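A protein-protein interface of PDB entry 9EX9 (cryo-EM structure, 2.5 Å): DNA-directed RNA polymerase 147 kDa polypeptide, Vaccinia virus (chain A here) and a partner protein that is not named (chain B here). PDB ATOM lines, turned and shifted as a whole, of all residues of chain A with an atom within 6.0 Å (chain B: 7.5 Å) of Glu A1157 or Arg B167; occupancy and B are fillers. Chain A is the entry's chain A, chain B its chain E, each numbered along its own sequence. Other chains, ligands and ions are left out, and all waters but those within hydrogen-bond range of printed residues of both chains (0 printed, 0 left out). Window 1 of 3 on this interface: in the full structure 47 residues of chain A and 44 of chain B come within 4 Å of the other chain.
OE1 of Glu A1157 lies within salt-bridge range of NE of Arg A1160 (3.6 Å). The guanidinium group of Arg A1160 lies within salt-bridge range of the side-chain carboxylate of Asp A1183 (2.8 Å). O of Ser B113 lies within hydrogen-bond range of N of Phe B166 (3.1 Å). The backbone carbonyl oxygen (O) of Arg B179 sits at hydrogen-bond distance from the backbone NH (N) of Val B163 (2.9 Å). The backbone NH (N) of Phe B165 sits at hydrogen-bond distance from the backbone carbonyl oxygen (O) of Ala B177 (2.9 Å). ND2 of Asn B169 lies within hydrogen-bond range of OE1 of Glu B175 (3.0 Å).
Of the 24 printed residues of chain B, 9 touch a printed residue of chain A. Hydrophobic or aromatic side chains of chain B within 4 Å of the printed part of chain A: Phe B165. Among the printed residues, Asp or Glu carboxylates within 4 Å of a Lys or Arg side-chain nitrogen of the other chain: Glu A1157 with Arg B167 (3.4 Å) and Glu A1157 with Arg B179 (3.5 Å).
The side-chain amide nitrogen (NE2) of Gln A822 lies within hydrogen-bond range of the backbone carbonyl oxygen (O) of Phe B166 (3.1 Å). The side-chain amide nitrogen of Gln A822 sits at hydrogen-bond distance from the side-chain amide oxygen of Asn B168. The side-chain carboxylate (OE1) of Glu A1157 lies within salt-bridge range of the guanidinium group (NE) of Arg B167. The side-chain carboxylate (OE2) of Glu A1157 lies within salt-bridge range of the guanidinium group (NE) of Arg B179, 3.5 Å away.
OE2 of Glu B175 touches CD of Lys A782, 3.4 Å away. Gln A822 touches Arg B167 (NE2 to O, 3.8 Å). Gln A822 touches Gly B173 (CG to O, 3.9 Å). Glu B147 touches Gly A1155 (OE2 to CA, 3.9 Å). Glu B147 touches Ile A1156 (OE2 to N, 3.6 Å). Ile A1156 touches Arg B179. Glu A1157 touches Phe B165 (OE2 to CD1, 3.9 Å). Ala A1158 touches Leu B110 (CB to O, 3.8 Å). NE of Arg A1160 touches CZ of Arg B167 (3.6 Å).
Of the printed residues of chain B, Gln A822 touches Phe B166 (3.1 Å), Arg B167 (3.8 Å), Asn B168 (2.5 Å) and Gly B173 (3.9 Å). Of the printed residues of chain B, Gly A1155 touches Glu B147 (3.9 Å). Glu A1157 touches just these residues of chain B: Phe B165 (3.9 Å), Arg B167 (3.4 Å) and Arg B179 (3.5 Å). Printed residues of chain B within 4 Å of Ala A1158: Leu B110. Val B149 touches none of the printed residues of chain A. Val B163 touches none of the printed residues of chain A. Of the printed residues of chain A, Phe B165 touches Glu A1157 (3.9 Å). Arg B167 touches just these residues of chain A: Gln A822, Glu A1157 and Arg A1160. The nearest residue of chain B that does not touch Glu A1157 is Ala B177 (4.3 Å). The nearest residue of chain A that does not touch Arg B167 is Ser A1187 (4.4 Å).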
ATOM      1  N   ILE A 781      10.208  35.588 -19.437  1.00  0.00           N
ATOM      2  CA  ILE A 781      10.023  34.243 -18.909  1.00  0.00           C
ATOM      3  C   ILE A 781      11.036  33.273 -19.497  1.00  0.00           C
ATOM      4  O   ILE A 781      11.646  32.490 -18.767  1.00  0.00           O
ATOM      5  CB  ILE A 781       8.579  33.769 -19.162  1.00  0.00           C
ATOM      6  CG1 ILE A 781       7.585  34.615 -18.365  1.00  0.00           C
ATOM      7  CG2 ILE A 781       8.428  32.303 -18.809  1.00  0.00           C
ATOM      8  CD1 ILE A 781       7.703  34.478 -16.862  1.00  0.00           C
ATOM      9  N   LYS A 782      11.244  33.300 -20.811  1.00  0.00           N
ATOM     10  CA  LYS A 782      12.147  32.344 -21.436  1.00  0.00           C
ATOM     11  C   LYS A 782      12.786  32.947 -22.675  1.00  0.00           C
ATOM     12  O   LYS A 782      12.114  33.605 -23.470  1.00  0.00           O
ATOM     13  CB  LYS A 782      11.410  31.056 -21.803  1.00  0.00           C
ATOM     14  CG  LYS A 782      12.308  29.971 -22.340  1.00  0.00           C
ATOM     15  CD  LYS A 782      11.814  28.596 -21.946  1.00  0.00           C
ATOM     16  CE  LYS A 782      10.419  28.334 -22.464  1.00  0.00           C
ATOM     17  NZ  LYS A 782       9.943  26.974 -22.107  1.00  0.00           N
ATOM     18  N   GLN A 822      23.918  16.495 -18.312  1.00  0.00           N
ATOM     19  CA  GLN A 822      23.462  16.625 -16.931  1.00  0.00           C
ATOM     20  C   GLN A 822      21.970  16.354 -16.807  1.00  0.00           C
ATOM     21  O   GLN A 822      21.526  15.723 -15.844  1.00  0.00           O
ATOM     22  CB  GLN A 822      23.806  18.010 -16.391  1.00  0.00           C
ATOM     23  CG  GLN A 822      23.074  19.148 -17.057  1.00  0.00           C
ATOM     24  CD  GLN A 822      23.505  20.495 -16.528  1.00  0.00           C
ATOM     25  OE1 GLN A 822      24.638  20.920 -16.735  1.00  0.00           O
ATOM     26  NE2 GLN A 822      22.604  21.173 -15.834  1.00  0.00           N
ATOM     27  N   GLY A1155      16.620  27.264  -2.926  1.00  0.00           N
ATOM     28  CA  GLY A1155      16.304  28.532  -3.541  1.00  0.00           C
ATOM     29  C   GLY A1155      15.069  28.432  -4.404  1.00  0.00           C
ATOM     30  O   GLY A1155      14.302  27.478  -4.318  1.00  0.00           O
ATOM     31  N   ILE A1156      14.893  29.442  -5.255  1.00  0.00           N
ATOM     32  CA  ILE A1156      13.693  29.535  -6.080  1.00  0.00           C
ATOM     33  C   ILE A1156      13.819  28.667  -7.327  1.00  0.00           C
ATOM     34  O   ILE A1156      12.832  28.090  -7.794  1.00  0.00           O
ATOM     35  CB  ILE A1156      13.418  31.012  -6.425  1.00  0.00           C
ATOM     36  CG1 ILE A1156      12.138  31.152  -7.247  1.00  0.00           C
ATOM     37  CG2 ILE A1156      14.593  31.628  -7.159  1.00  0.00           C
ATOM     38  CD1 ILE A1156      10.905  30.746  -6.506  1.00  0.00           C
ATOM     39  N   GLU A1157      15.023  28.558  -7.888  1.00  0.00           N
ATOM     40  CA  GLU A1157      15.212  27.711  -9.061  1.00  0.00           C
ATOM     41  C   GLU A1157      14.933  26.248  -8.740  1.00  0.00           C
ATOM     42  O   GLU A1157      14.299  25.536  -9.532  1.00  0.00           O
ATOM     43  CB  GLU A1157      16.628  27.885  -9.603  1.00  0.00           C
ATOM     44  CG  GLU A1157      16.845  29.172 -10.377  1.00  0.00           C
ATOM     45  CD  GLU A1157      16.174  29.161 -11.740  1.00  0.00           C
ATOM     46  OE1 GLU A1157      15.467  28.187 -12.054  1.00  0.00           O
ATOM     47  OE2 GLU A1157      16.359  30.127 -12.504  1.00  0.00           O
ATOM     48  N   ALA A1158      15.401  25.777  -7.583  1.00  0.00           N
ATOM     49  CA  ALA A1158      15.124  24.402  -7.185  1.00  0.00           C
ATOM     50  C   ALA A1158      13.632  24.179  -6.992  1.00  0.00           C
ATOM     51  O   ALA A1158      13.101  23.125  -7.358  1.00  0.00           O
ATOM     52  CB  ALA A1158      15.885  24.067  -5.906  1.00  0.00           C
ATOM     53  N   ALA A1159      12.940  25.157  -6.411  1.00  0.00           N
ATOM     54  CA  ALA A1159      11.494  25.047  -6.260  1.00  0.00           C
ATOM     55  C   ALA A1159      10.807  24.958  -7.614  1.00  0.00           C
ATOM     56  O   ALA A1159       9.871  24.170  -7.797  1.00  0.00           O
ATOM     57  CB  ALA A1159      10.964  26.237  -5.466  1.00  0.00           C
ATOM     58  N   ARG A1160      11.259  25.759  -8.578  1.00  0.00           N
ATOM     59  CA  ARG A1160      10.685  25.704  -9.918  1.00  0.00           C
ATOM     60  C   ARG A1160      10.886  24.328 -10.538  1.00  0.00           C
ATOM     61  O   ARG A1160       9.962  23.759 -11.136  1.00  0.00           O
ATOM     62  CB  ARG A1160      11.317  26.790 -10.788  1.00  0.00           C
ATOM     63  CG  ARG A1160      10.593  27.040 -12.097  1.00  0.00           C
ATOM     64  CD  ARG A1160      11.534  27.555 -13.158  1.00  0.00           C
ATOM     65  NE  ARG A1160      12.572  26.580 -13.460  1.00  0.00           N
ATOM     66  CZ  ARG A1160      12.417  25.546 -14.275  1.00  0.00           C
ATOM     67  NH1 ARG A1160      11.283  25.334 -14.918  1.00  0.00           N
ATOM     68  NH2 ARG A1160      13.425  24.695 -14.438  1.00  0.00           N
ATOM     69  N   GLU A1161      12.095  23.779 -10.408  1.00  0.00           N
ATOM     70  CA  GLU A1161      12.369  22.457 -10.963  1.00  0.00           C
ATOM     71  C   GLU A1161      11.485  21.399 -10.318  1.00  0.00           C
ATOM     72  O   GLU A1161      10.909  20.540 -11.002  1.00  0.00           O
ATOM     73  CB  GLU A1161      13.842  22.108 -10.772  1.00  0.00           C
ATOM     74  CG  GLU A1161      14.243  20.772 -11.371  1.00  0.00           C
ATOM     75  CD  GLU A1161      15.645  20.358 -10.991  1.00  0.00           C
ATOM     76  OE1 GLU A1161      16.383  21.193 -10.437  1.00  0.00           O
ATOM     77  OE2 GLU A1161      16.009  19.192 -11.242  1.00  0.00           O
ATOM     78  N   TYR A1162      11.373  21.443  -8.990  1.00  0.00           N
ATOM     79  CA  TYR A1162      10.533  20.480  -8.294  1.00  0.00           C
ATOM     80  C   TYR A1162       9.096  20.566  -8.778  1.00  0.00           C
ATOM     81  O   TYR A1162       8.453  19.541  -9.028  1.00  0.00           O
ATOM     82  CB  TYR A1162      10.603  20.712  -6.784  1.00  0.00           C
ATOM     83  CG  TYR A1162       9.686  19.799  -6.008  1.00  0.00           C
ATOM     84  CD1 TYR A1162      10.124  18.563  -5.558  1.00  0.00           C
ATOM     85  CD2 TYR A1162       8.377  20.162  -5.746  1.00  0.00           C
ATOM     86  CE1 TYR A1162       9.286  17.722  -4.865  1.00  0.00           C
ATOM     87  CE2 TYR A1162       7.534  19.328  -5.057  1.00  0.00           C
ATOM     88  CZ  TYR A1162       7.991  18.109  -4.619  1.00  0.00           C
ATOM     89  OH  TYR A1162       7.144  17.280  -3.928  1.00  0.00           O
ATOM     90  N   ASP A1183       6.591  23.111 -17.929  1.00  0.00           N
ATOM     91  CA  ASP A1183       7.750  23.967 -17.714  1.00  0.00           C
ATOM     92  C   ASP A1183       7.371  25.438 -17.769  1.00  0.00           C
ATOM     93  O   ASP A1183       7.972  26.266 -17.080  1.00  0.00           O
ATOM     94  CB  ASP A1183       8.823  23.651 -18.753  1.00  0.00           C
ATOM     95  CG  ASP A1183      10.096  24.417 -18.522  1.00  0.00           C
ATOM     96  OD1 ASP A1183      10.183  25.130 -17.508  1.00  0.00           O
ATOM     97  OD2 ASP A1183      11.013  24.303 -19.356  1.00  0.00           O
ATOM     98  N   SER A1187       7.333  27.910 -14.460  1.00  0.00           N
ATOM     99  CA  SER A1187       8.103  29.136 -14.599  1.00  0.00           C
ATOM    100  C   SER A1187       7.253  30.354 -14.288  1.00  0.00           C
ATOM    101  O   SER A1187       7.784  31.398 -13.902  1.00  0.00           O
ATOM    102  CB  SER A1187       8.679  29.238 -16.008  1.00  0.00           C
ATOM    103  OG  SER A1187       9.448  28.093 -16.319  1.00  0.00           O
ATOM    104  N   LEU B 110      19.398  18.421  -6.021  1.00  0.00           N
ATOM    105  CA  LEU B 110      18.701  19.687  -6.173  1.00  0.00           C
ATOM    106  C   LEU B 110      19.611  20.896  -6.011  1.00  0.00           C
ATOM    107  O   LEU B 110      19.134  22.026  -6.131  1.00  0.00           O
ATOM    108  CB  LEU B 110      17.551  19.763  -5.169  1.00  0.00           C
ATOM    109  CG  LEU B 110      16.400  18.807  -5.473  1.00  0.00           C
ATOM    110  CD1 LEU B 110      15.711  18.369  -4.207  1.00  0.00           C
ATOM    111  CD2 LEU B 110      15.405  19.458  -6.411  1.00  0.00           C
ATOM    112  N   PRO B 112      21.974  23.753  -7.186  1.00  0.00           N
ATOM    113  CA  PRO B 112      22.012  24.355  -8.521  1.00  0.00           C
ATOM    114  C   PRO B 112      23.402  24.301  -9.141  1.00  0.00           C
ATOM    115  O   PRO B 112      24.383  23.888  -8.524  1.00  0.00           O
ATOM    116  CB  PRO B 112      21.587  25.808  -8.274  1.00  0.00           C
ATOM    117  CG  PRO B 112      21.123  25.868  -6.874  1.00  0.00           C
ATOM    118  CD  PRO B 112      21.825  24.785  -6.150  1.00  0.00           C
ATOM    119  N   SER B 113      23.456  24.722 -10.403  1.00  0.00           N
ATOM    120  CA  SER B 113      24.695  25.014 -11.112  1.00  0.00           C
ATOM    121  C   SER B 113      24.595  26.445 -11.614  1.00  0.00           C
ATOM    122  O   SER B 113      23.663  26.778 -12.350  1.00  0.00           O
ATOM    123  CB  SER B 113      24.909  24.043 -12.271  1.00  0.00           C
ATOM    124  OG  SER B 113      26.084  24.362 -12.987  1.00  0.00           O
ATOM    125  N   PRO B 141      13.554  37.763 -14.006  1.00  0.00           N
ATOM    126  CA  PRO B 141      12.945  37.358 -12.736  1.00  0.00           C
ATOM    127  C   PRO B 141      13.889  37.617 -11.572  1.00  0.00           C
ATOM    128  O   PRO B 141      15.063  37.946 -11.743  1.00  0.00           O
ATOM    129  CB  PRO B 141      12.669  35.868 -12.935  1.00  0.00           C
ATOM    130  CG  PRO B 141      12.538  35.711 -14.396  1.00  0.00           C
ATOM    131  CD  PRO B 141      13.491  36.687 -15.006  1.00  0.00           C
ATOM    132  N   LYS B 142      13.356  37.463 -10.364  1.00  0.00           N
ATOM    133  CA  LYS B 142      14.012  37.933  -9.153  1.00  0.00           C
ATOM    134  C   LYS B 142      14.456  36.778  -8.267  1.00  0.00           C
ATOM    135  O   LYS B 142      13.927  35.668  -8.336  1.00  0.00           O
ATOM    136  CB  LYS B 142      13.078  38.845  -8.356  1.00  0.00           C
ATOM    137  CG  LYS B 142      12.630  40.083  -9.097  1.00  0.00           C
ATOM    138  CD  LYS B 142      11.652  40.880  -8.263  1.00  0.00           C
ATOM    139  CE  LYS B 142      11.146  42.097  -9.008  1.00  0.00           C
ATOM    140  NZ  LYS B 142      10.136  42.846  -8.212  1.00  0.00           N
ATOM    141  N   MET B 143      15.441  37.070  -7.422  1.00  0.00           N
ATOM    142  CA  MET B 143      15.887  36.160  -6.379  1.00  0.00           C
ATOM    143  C   MET B 143      16.426  36.988  -5.223  1.00  0.00           C
ATOM    144  O   MET B 143      17.068  38.018  -5.429  1.00  0.00           O
ATOM    145  CB  MET B 143      16.960  35.197  -6.890  1.00  0.00           C
ATOM    146  CG  MET B 143      18.275  35.862  -7.228  1.00  0.00           C
ATOM    147  SD  MET B 143      19.476  34.721  -7.920  1.00  0.00           S
ATOM    148  CE  MET B 143      19.603  33.536  -6.597  1.00  0.00           C
ATOM    149  N   GLU B 147      20.018  34.166  -0.341  1.00  0.00           N
ATOM    150  CA  GLU B 147      20.122  32.769  -0.730  1.00  0.00           C
ATOM    151  C   GLU B 147      21.563  32.283  -0.614  1.00  0.00           C
ATOM    152  O   GLU B 147      22.513  33.065  -0.651  1.00  0.00           O
ATOM    153  CB  GLU B 147      19.615  32.573  -2.158  1.00  0.00           C
ATOM    154  CG  GLU B 147      18.153  32.920  -2.331  1.00  0.00           C
ATOM    155  CD  GLU B 147      17.585  32.405  -3.631  1.00  0.00           C
ATOM    156  OE1 GLU B 147      18.372  31.963  -4.485  1.00  0.00           O
ATOM    157  OE2 GLU B 147      16.349  32.435  -3.796  1.00  0.00           O
ATOM    158  N   VAL B 149      23.197  30.644  -2.740  1.00  0.00           N
ATOM    159  CA  VAL B 149      23.894  30.918  -3.992  1.00  0.00           C
ATOM    160  C   VAL B 149      24.641  32.238  -3.899  1.00  0.00           C
ATOM    161  O   VAL B 149      25.819  32.336  -4.257  1.00  0.00           O
ATOM    162  CB  VAL B 149      22.896  30.921  -5.163  1.00  0.00           C
ATOM    163  CG1 VAL B 149      23.537  31.500  -6.400  1.00  0.00           C
ATOM    164  CG2 VAL B 149      22.393  29.526  -5.427  1.00  0.00           C
ATOM    165  N   VAL B 163      22.802  36.565 -12.003  1.00  0.00           N
ATOM    166  CA  VAL B 163      23.344  35.224 -11.819  1.00  0.00           C
ATOM    167  C   VAL B 163      22.768  34.327 -12.904  1.00  0.00           C
ATOM    168  O   VAL B 163      21.559  34.362 -13.163  1.00  0.00           O
ATOM    169  CB  VAL B 163      23.021  34.664 -10.423  1.00  0.00           C
ATOM    170  CG1 VAL B 163      23.744  33.353 -10.204  1.00  0.00           C
ATOM    171  CG2 VAL B 163      23.404  35.659  -9.353  1.00  0.00           C
ATOM    172  N   ARG B 164      23.628  33.525 -13.533  1.00  0.00           N
ATOM    173  CA  ARG B 164      23.230  32.656 -14.631  1.00  0.00           C
ATOM    174  C   ARG B 164      23.167  31.212 -14.158  1.00  0.00           C
ATOM    175  O   ARG B 164      24.122  30.711 -13.557  1.00  0.00           O
ATOM    176  CB  ARG B 164      24.205  32.786 -15.799  1.00  0.00           C
ATOM    177  CG  ARG B 164      24.007  31.751 -16.884  1.00  0.00           C
ATOM    178  CD  ARG B 164      24.705  32.160 -18.157  1.00  0.00           C
ATOM    179  NE  ARG B 164      24.037  33.275 -18.814  1.00  0.00           N
ATOM    180  CZ  ARG B 164      24.496  33.890 -19.895  1.00  0.00           C
ATOM    181  NH1 ARG B 164      25.638  33.535 -20.459  1.00  0.00           N
ATOM    182  NH2 ARG B 164      23.793  34.887 -20.421  1.00  0.00           N
ATOM    183  N   PHE B 165      22.053  30.545 -14.445  1.00  0.00           N
ATOM    184  CA  PHE B 165      21.808  29.170 -14.038  1.00  0.00           C
ATOM    185  C   PHE B 165      21.762  28.249 -15.250  1.00  0.00           C
ATOM    186  O   PHE B 165      21.140  28.574 -16.268  1.00  0.00           O
ATOM    187  CB  PHE B 165      20.488  29.049 -13.274  1.00  0.00           C
ATOM    188  CG  PHE B 165      20.465  29.796 -11.978  1.00  0.00           C
ATOM    189  CD1 PHE B 165      20.101  31.125 -11.936  1.00  0.00           C
ATOM    190  CD2 PHE B 165      20.801  29.168 -10.798  1.00  0.00           C
ATOM    191  CE1 PHE B 165      20.081  31.807 -10.750  1.00  0.00           C
ATOM    192  CE2 PHE B 165      20.780  29.850  -9.611  1.00  0.00           C
ATOM    193  CZ  PHE B 165      20.419  31.168  -9.587  1.00  0.00           C
ATOM    194  N   PHE B 166      22.414  27.094 -15.122  1.00  0.00           N
ATOM    195  CA  PHE B 166      22.386  26.036 -16.129  1.00  0.00           C
ATOM    196  C   PHE B 166      21.395  24.975 -15.662  1.00  0.00           C
ATOM    197  O   PHE B 166      21.754  24.017 -14.981  1.00  0.00           O
ATOM    198  CB  PHE B 166      23.773  25.451 -16.342  1.00  0.00           C
ATOM    199  CG  PHE B 166      24.811  26.475 -16.677  1.00  0.00           C
ATOM    200  CD1 PHE B 166      24.985  26.897 -17.975  1.00  0.00           C
ATOM    201  CD2 PHE B 166      25.609  27.015 -15.695  1.00  0.00           C
ATOM    202  CE1 PHE B 166      25.935  27.840 -18.283  1.00  0.00           C
ATOM    203  CE2 PHE B 166      26.560  27.956 -16.002  1.00  0.00           C
ATOM    204  CZ  PHE B 166      26.721  28.368 -17.296  1.00  0.00           C
ATOM    205  N   ARG B 167      20.136  25.154 -16.041  1.00  0.00           N
ATOM    206  CA  ARG B 167      19.079  24.242 -15.633  1.00  0.00           C
ATOM    207  C   ARG B 167      19.229  22.887 -16.304  1.00  0.00           C
ATOM    208  O   ARG B 167      19.633  22.794 -17.464  1.00  0.00           O
ATOM    209  CB  ARG B 167      17.714  24.814 -15.998  1.00  0.00           C
ATOM    210  CG  ARG B 167      17.428  26.203 -15.493  1.00  0.00           C
ATOM    211  CD  ARG B 167      16.132  26.692 -16.096  1.00  0.00           C
ATOM    212  NE  ARG B 167      15.619  27.894 -15.456  1.00  0.00           N
ATOM    213  CZ  ARG B 167      14.521  28.528 -15.839  1.00  0.00           C
ATOM    214  NH1 ARG B 167      13.808  28.114 -16.872  1.00  0.00           N
ATOM    215  NH2 ARG B 167      14.122  29.600 -15.163  1.00  0.00           N
ATOM    216  N   ASN B 168      18.877  21.834 -15.571  1.00  0.00           N
ATOM    217  CA  ASN B 168      18.687  20.524 -16.177  1.00  0.00           C
ATOM    218  C   ASN B 168      17.407  20.528 -16.994  1.00  0.00           C
ATOM    219  O   ASN B 168      16.352  20.935 -16.504  1.00  0.00           O
ATOM    220  CB  ASN B 168      18.608  19.440 -15.109  1.00  0.00           C
ATOM    221  CG  ASN B 168      19.826  19.399 -14.229  1.00  0.00           C
ATOM    222  OD1 ASN B 168      20.856  19.981 -14.551  1.00  0.00           O
ATOM    223  ND2 ASN B 168      19.721  18.696 -13.115  1.00  0.00           N
ATOM    224  N   ASN B 169      17.489  20.061 -18.233  1.00  0.00           N
ATOM    225  CA  ASN B 169      16.344  20.023 -19.125  1.00  0.00           C
ATOM    226  C   ASN B 169      16.204  18.609 -19.654  1.00  0.00           C
ATOM    227  O   ASN B 169      17.177  18.027 -20.140  1.00  0.00           O
ATOM    228  CB  ASN B 169      16.511  21.012 -20.274  1.00  0.00           C
ATOM    229  CG  ASN B 169      15.200  21.377 -20.915  1.00  0.00           C
ATOM    230  OD1 ASN B 169      14.693  20.659 -21.767  1.00  0.00           O
ATOM    231  ND2 ASN B 169      14.638  22.501 -20.506  1.00  0.00           N
ATOM    232  N   MET B 170      14.993  18.063 -19.569  1.00  0.00           N
ATOM    233  CA  MET B 170      14.795  16.658 -19.890  1.00  0.00           C
ATOM    234  C   MET B 170      14.953  16.384 -21.379  1.00  0.00           C
ATOM    235  O   MET B 170      15.349  15.278 -21.760  1.00  0.00           O
ATOM    236  CB  MET B 170      13.414  16.214 -19.417  1.00  0.00           C
ATOM    237  CG  MET B 170      13.197  14.724 -19.443  1.00  0.00           C
ATOM    238  SD  MET B 170      11.500  14.275 -19.053  1.00  0.00           S
ATOM    239  CE  MET B 170      10.678  14.749 -20.561  1.00  0.00           C
ATOM    240  N   THR B 172      16.479  18.769 -23.814  1.00  0.00           N
ATOM    241  CA  THR B 172      17.652  19.369 -24.434  1.00  0.00           C
ATOM    242  C   THR B 172      18.921  19.202 -23.613  1.00  0.00           C
ATOM    243  O   THR B 172      19.979  19.662 -24.047  1.00  0.00           O
ATOM    244  CB  THR B 172      17.425  20.861 -24.701  1.00  0.00           C
ATOM    245  OG1 THR B 172      17.523  21.597 -23.479  1.00  0.00           O
ATOM    246  CG2 THR B 172      16.069  21.101 -25.320  1.00  0.00           C
ATOM    247  N   GLY B 173      18.855  18.559 -22.454  1.00  0.00           N
ATOM    248  CA  GLY B 173      20.037  18.384 -21.635  1.00  0.00           C
ATOM    249  C   GLY B 173      20.273  19.542 -20.694  1.00  0.00           C
ATOM    250  O   GLY B 173      20.002  19.439 -19.498  1.00  0.00           O
ATOM    251  N   VAL B 174      20.739  20.667 -21.225  1.00  0.00           N
ATOM    252  CA  VAL B 174      21.024  21.847 -20.425  1.00  0.00           C
ATOM    253  C   VAL B 174      20.282  23.034 -21.018  1.00  0.00           C
ATOM    254  O   VAL B 174      20.061  23.109 -22.228  1.00  0.00           O
ATOM    255  CB  VAL B 174      22.533  22.135 -20.353  1.00  0.00           C
ATOM    256  CG1 VAL B 174      23.079  22.423 -21.728  1.00  0.00           C
ATOM    257  CG2 VAL B 174      22.799  23.293 -19.431  1.00  0.00           C
ATOM    258  N   GLU B 175      19.886  23.959 -20.148  1.00  0.00           N
ATOM    259  CA  GLU B 175      19.234  25.196 -20.553  1.00  0.00           C
ATOM    260  C   GLU B 175      19.836  26.346 -19.760  1.00  0.00           C
ATOM    261  O   GLU B 175      20.389  26.146 -18.684  1.00  0.00           O
ATOM    262  CB  GLU B 175      17.725  25.128 -20.323  1.00  0.00           C
ATOM    263  CG  GLU B 175      16.963  26.273 -20.927  1.00  0.00           C
ATOM    264  CD  GLU B 175      15.501  26.239 -20.573  1.00  0.00           C
ATOM    265  OE1 GLU B 175      15.104  25.366 -19.777  1.00  0.00           O
ATOM    266  OE2 GLU B 175      14.746  27.087 -21.082  1.00  0.00           O
ATOM    267  N   ILE B 176      19.737  27.559 -20.293  1.00  0.00           N
ATOM    268  CA  ILE B 176      20.334  28.736 -19.670  1.00  0.00           C
ATOM    269  C   ILE B 176      19.229  29.690 -19.244  1.00  0.00           C
ATOM    270  O   ILE B 176      18.338  30.013 -20.036  1.00  0.00           O
ATOM    271  CB  ILE B 176      21.326  29.432 -20.615  1.00  0.00           C
ATOM    272  CG1 ILE B 176      22.552  28.546 -20.816  1.00  0.00           C
ATOM    273  CG2 ILE B 176      21.720  30.788 -20.058  1.00  0.00           C
ATOM    274  CD1 ILE B 176      23.581  29.123 -21.745  1.00  0.00           C
ATOM    275  N   ALA B 177      19.293  30.144 -17.993  1.00  0.00           N
ATOM    276  CA  ALA B 177      18.381  31.159 -17.487  1.00  0.00           C
ATOM    277  C   ALA B 177      19.173  32.162 -16.663  1.00  0.00           C
ATOM    278  O   ALA B 177      20.314  31.908 -16.283  1.00  0.00           O
ATOM    279  CB  ALA B 177      17.261  30.542 -16.647  1.00  0.00           C
ATOM    280  N   ASP B 178      18.562  33.311 -16.389  1.00  0.00           N
ATOM    281  CA  ASP B 178      19.225  34.361 -15.629  1.00  0.00           C
ATOM    282  C   ASP B 178      18.266  34.941 -14.601  1.00  0.00           C
ATOM    283  O   ASP B 178      17.053  34.965 -14.809  1.00  0.00           O
ATOM    284  CB  ASP B 178      19.737  35.473 -16.545  1.00  0.00           C
ATOM    285  CG  ASP B 178      20.652  34.954 -17.628  1.00  0.00           C
ATOM    286  OD1 ASP B 178      21.425  34.018 -17.352  1.00  0.00           O
ATOM    287  OD2 ASP B 178      20.595  35.473 -18.760  1.00  0.00           O
ATOM    288  N   ARG B 179      18.829  35.406 -13.486  1.00  0.00           N
ATOM    289  CA  ARG B 179      18.053  36.021 -12.418  1.00  0.00           C
ATOM    290  C   ARG B 179      18.765  37.271 -11.933  1.00  0.00           C
ATOM    291  O   ARG B 179      19.988  37.387 -12.037  1.00  0.00           O
ATOM    292  CB  ARG B 179      17.844  35.072 -11.230  1.00  0.00           C
ATOM    293  CG  ARG B 179      16.952  33.886 -11.515  1.00  0.00           C
ATOM    294  CD  ARG B 179      15.582  34.065 -10.929  1.00  0.00           C
ATOM    295  NE  ARG B 179      14.738  32.907 -11.179  1.00  0.00           N
ATOM    296  CZ  ARG B 179      13.483  32.791 -10.773  1.00  0.00           C
ATOM    297  NH1 ARG B 179      12.887  33.752 -10.091  1.00  0.00           N
ATOM    298  NH2 ARG B 179      12.807  31.687 -11.062  1.00  0.00           N
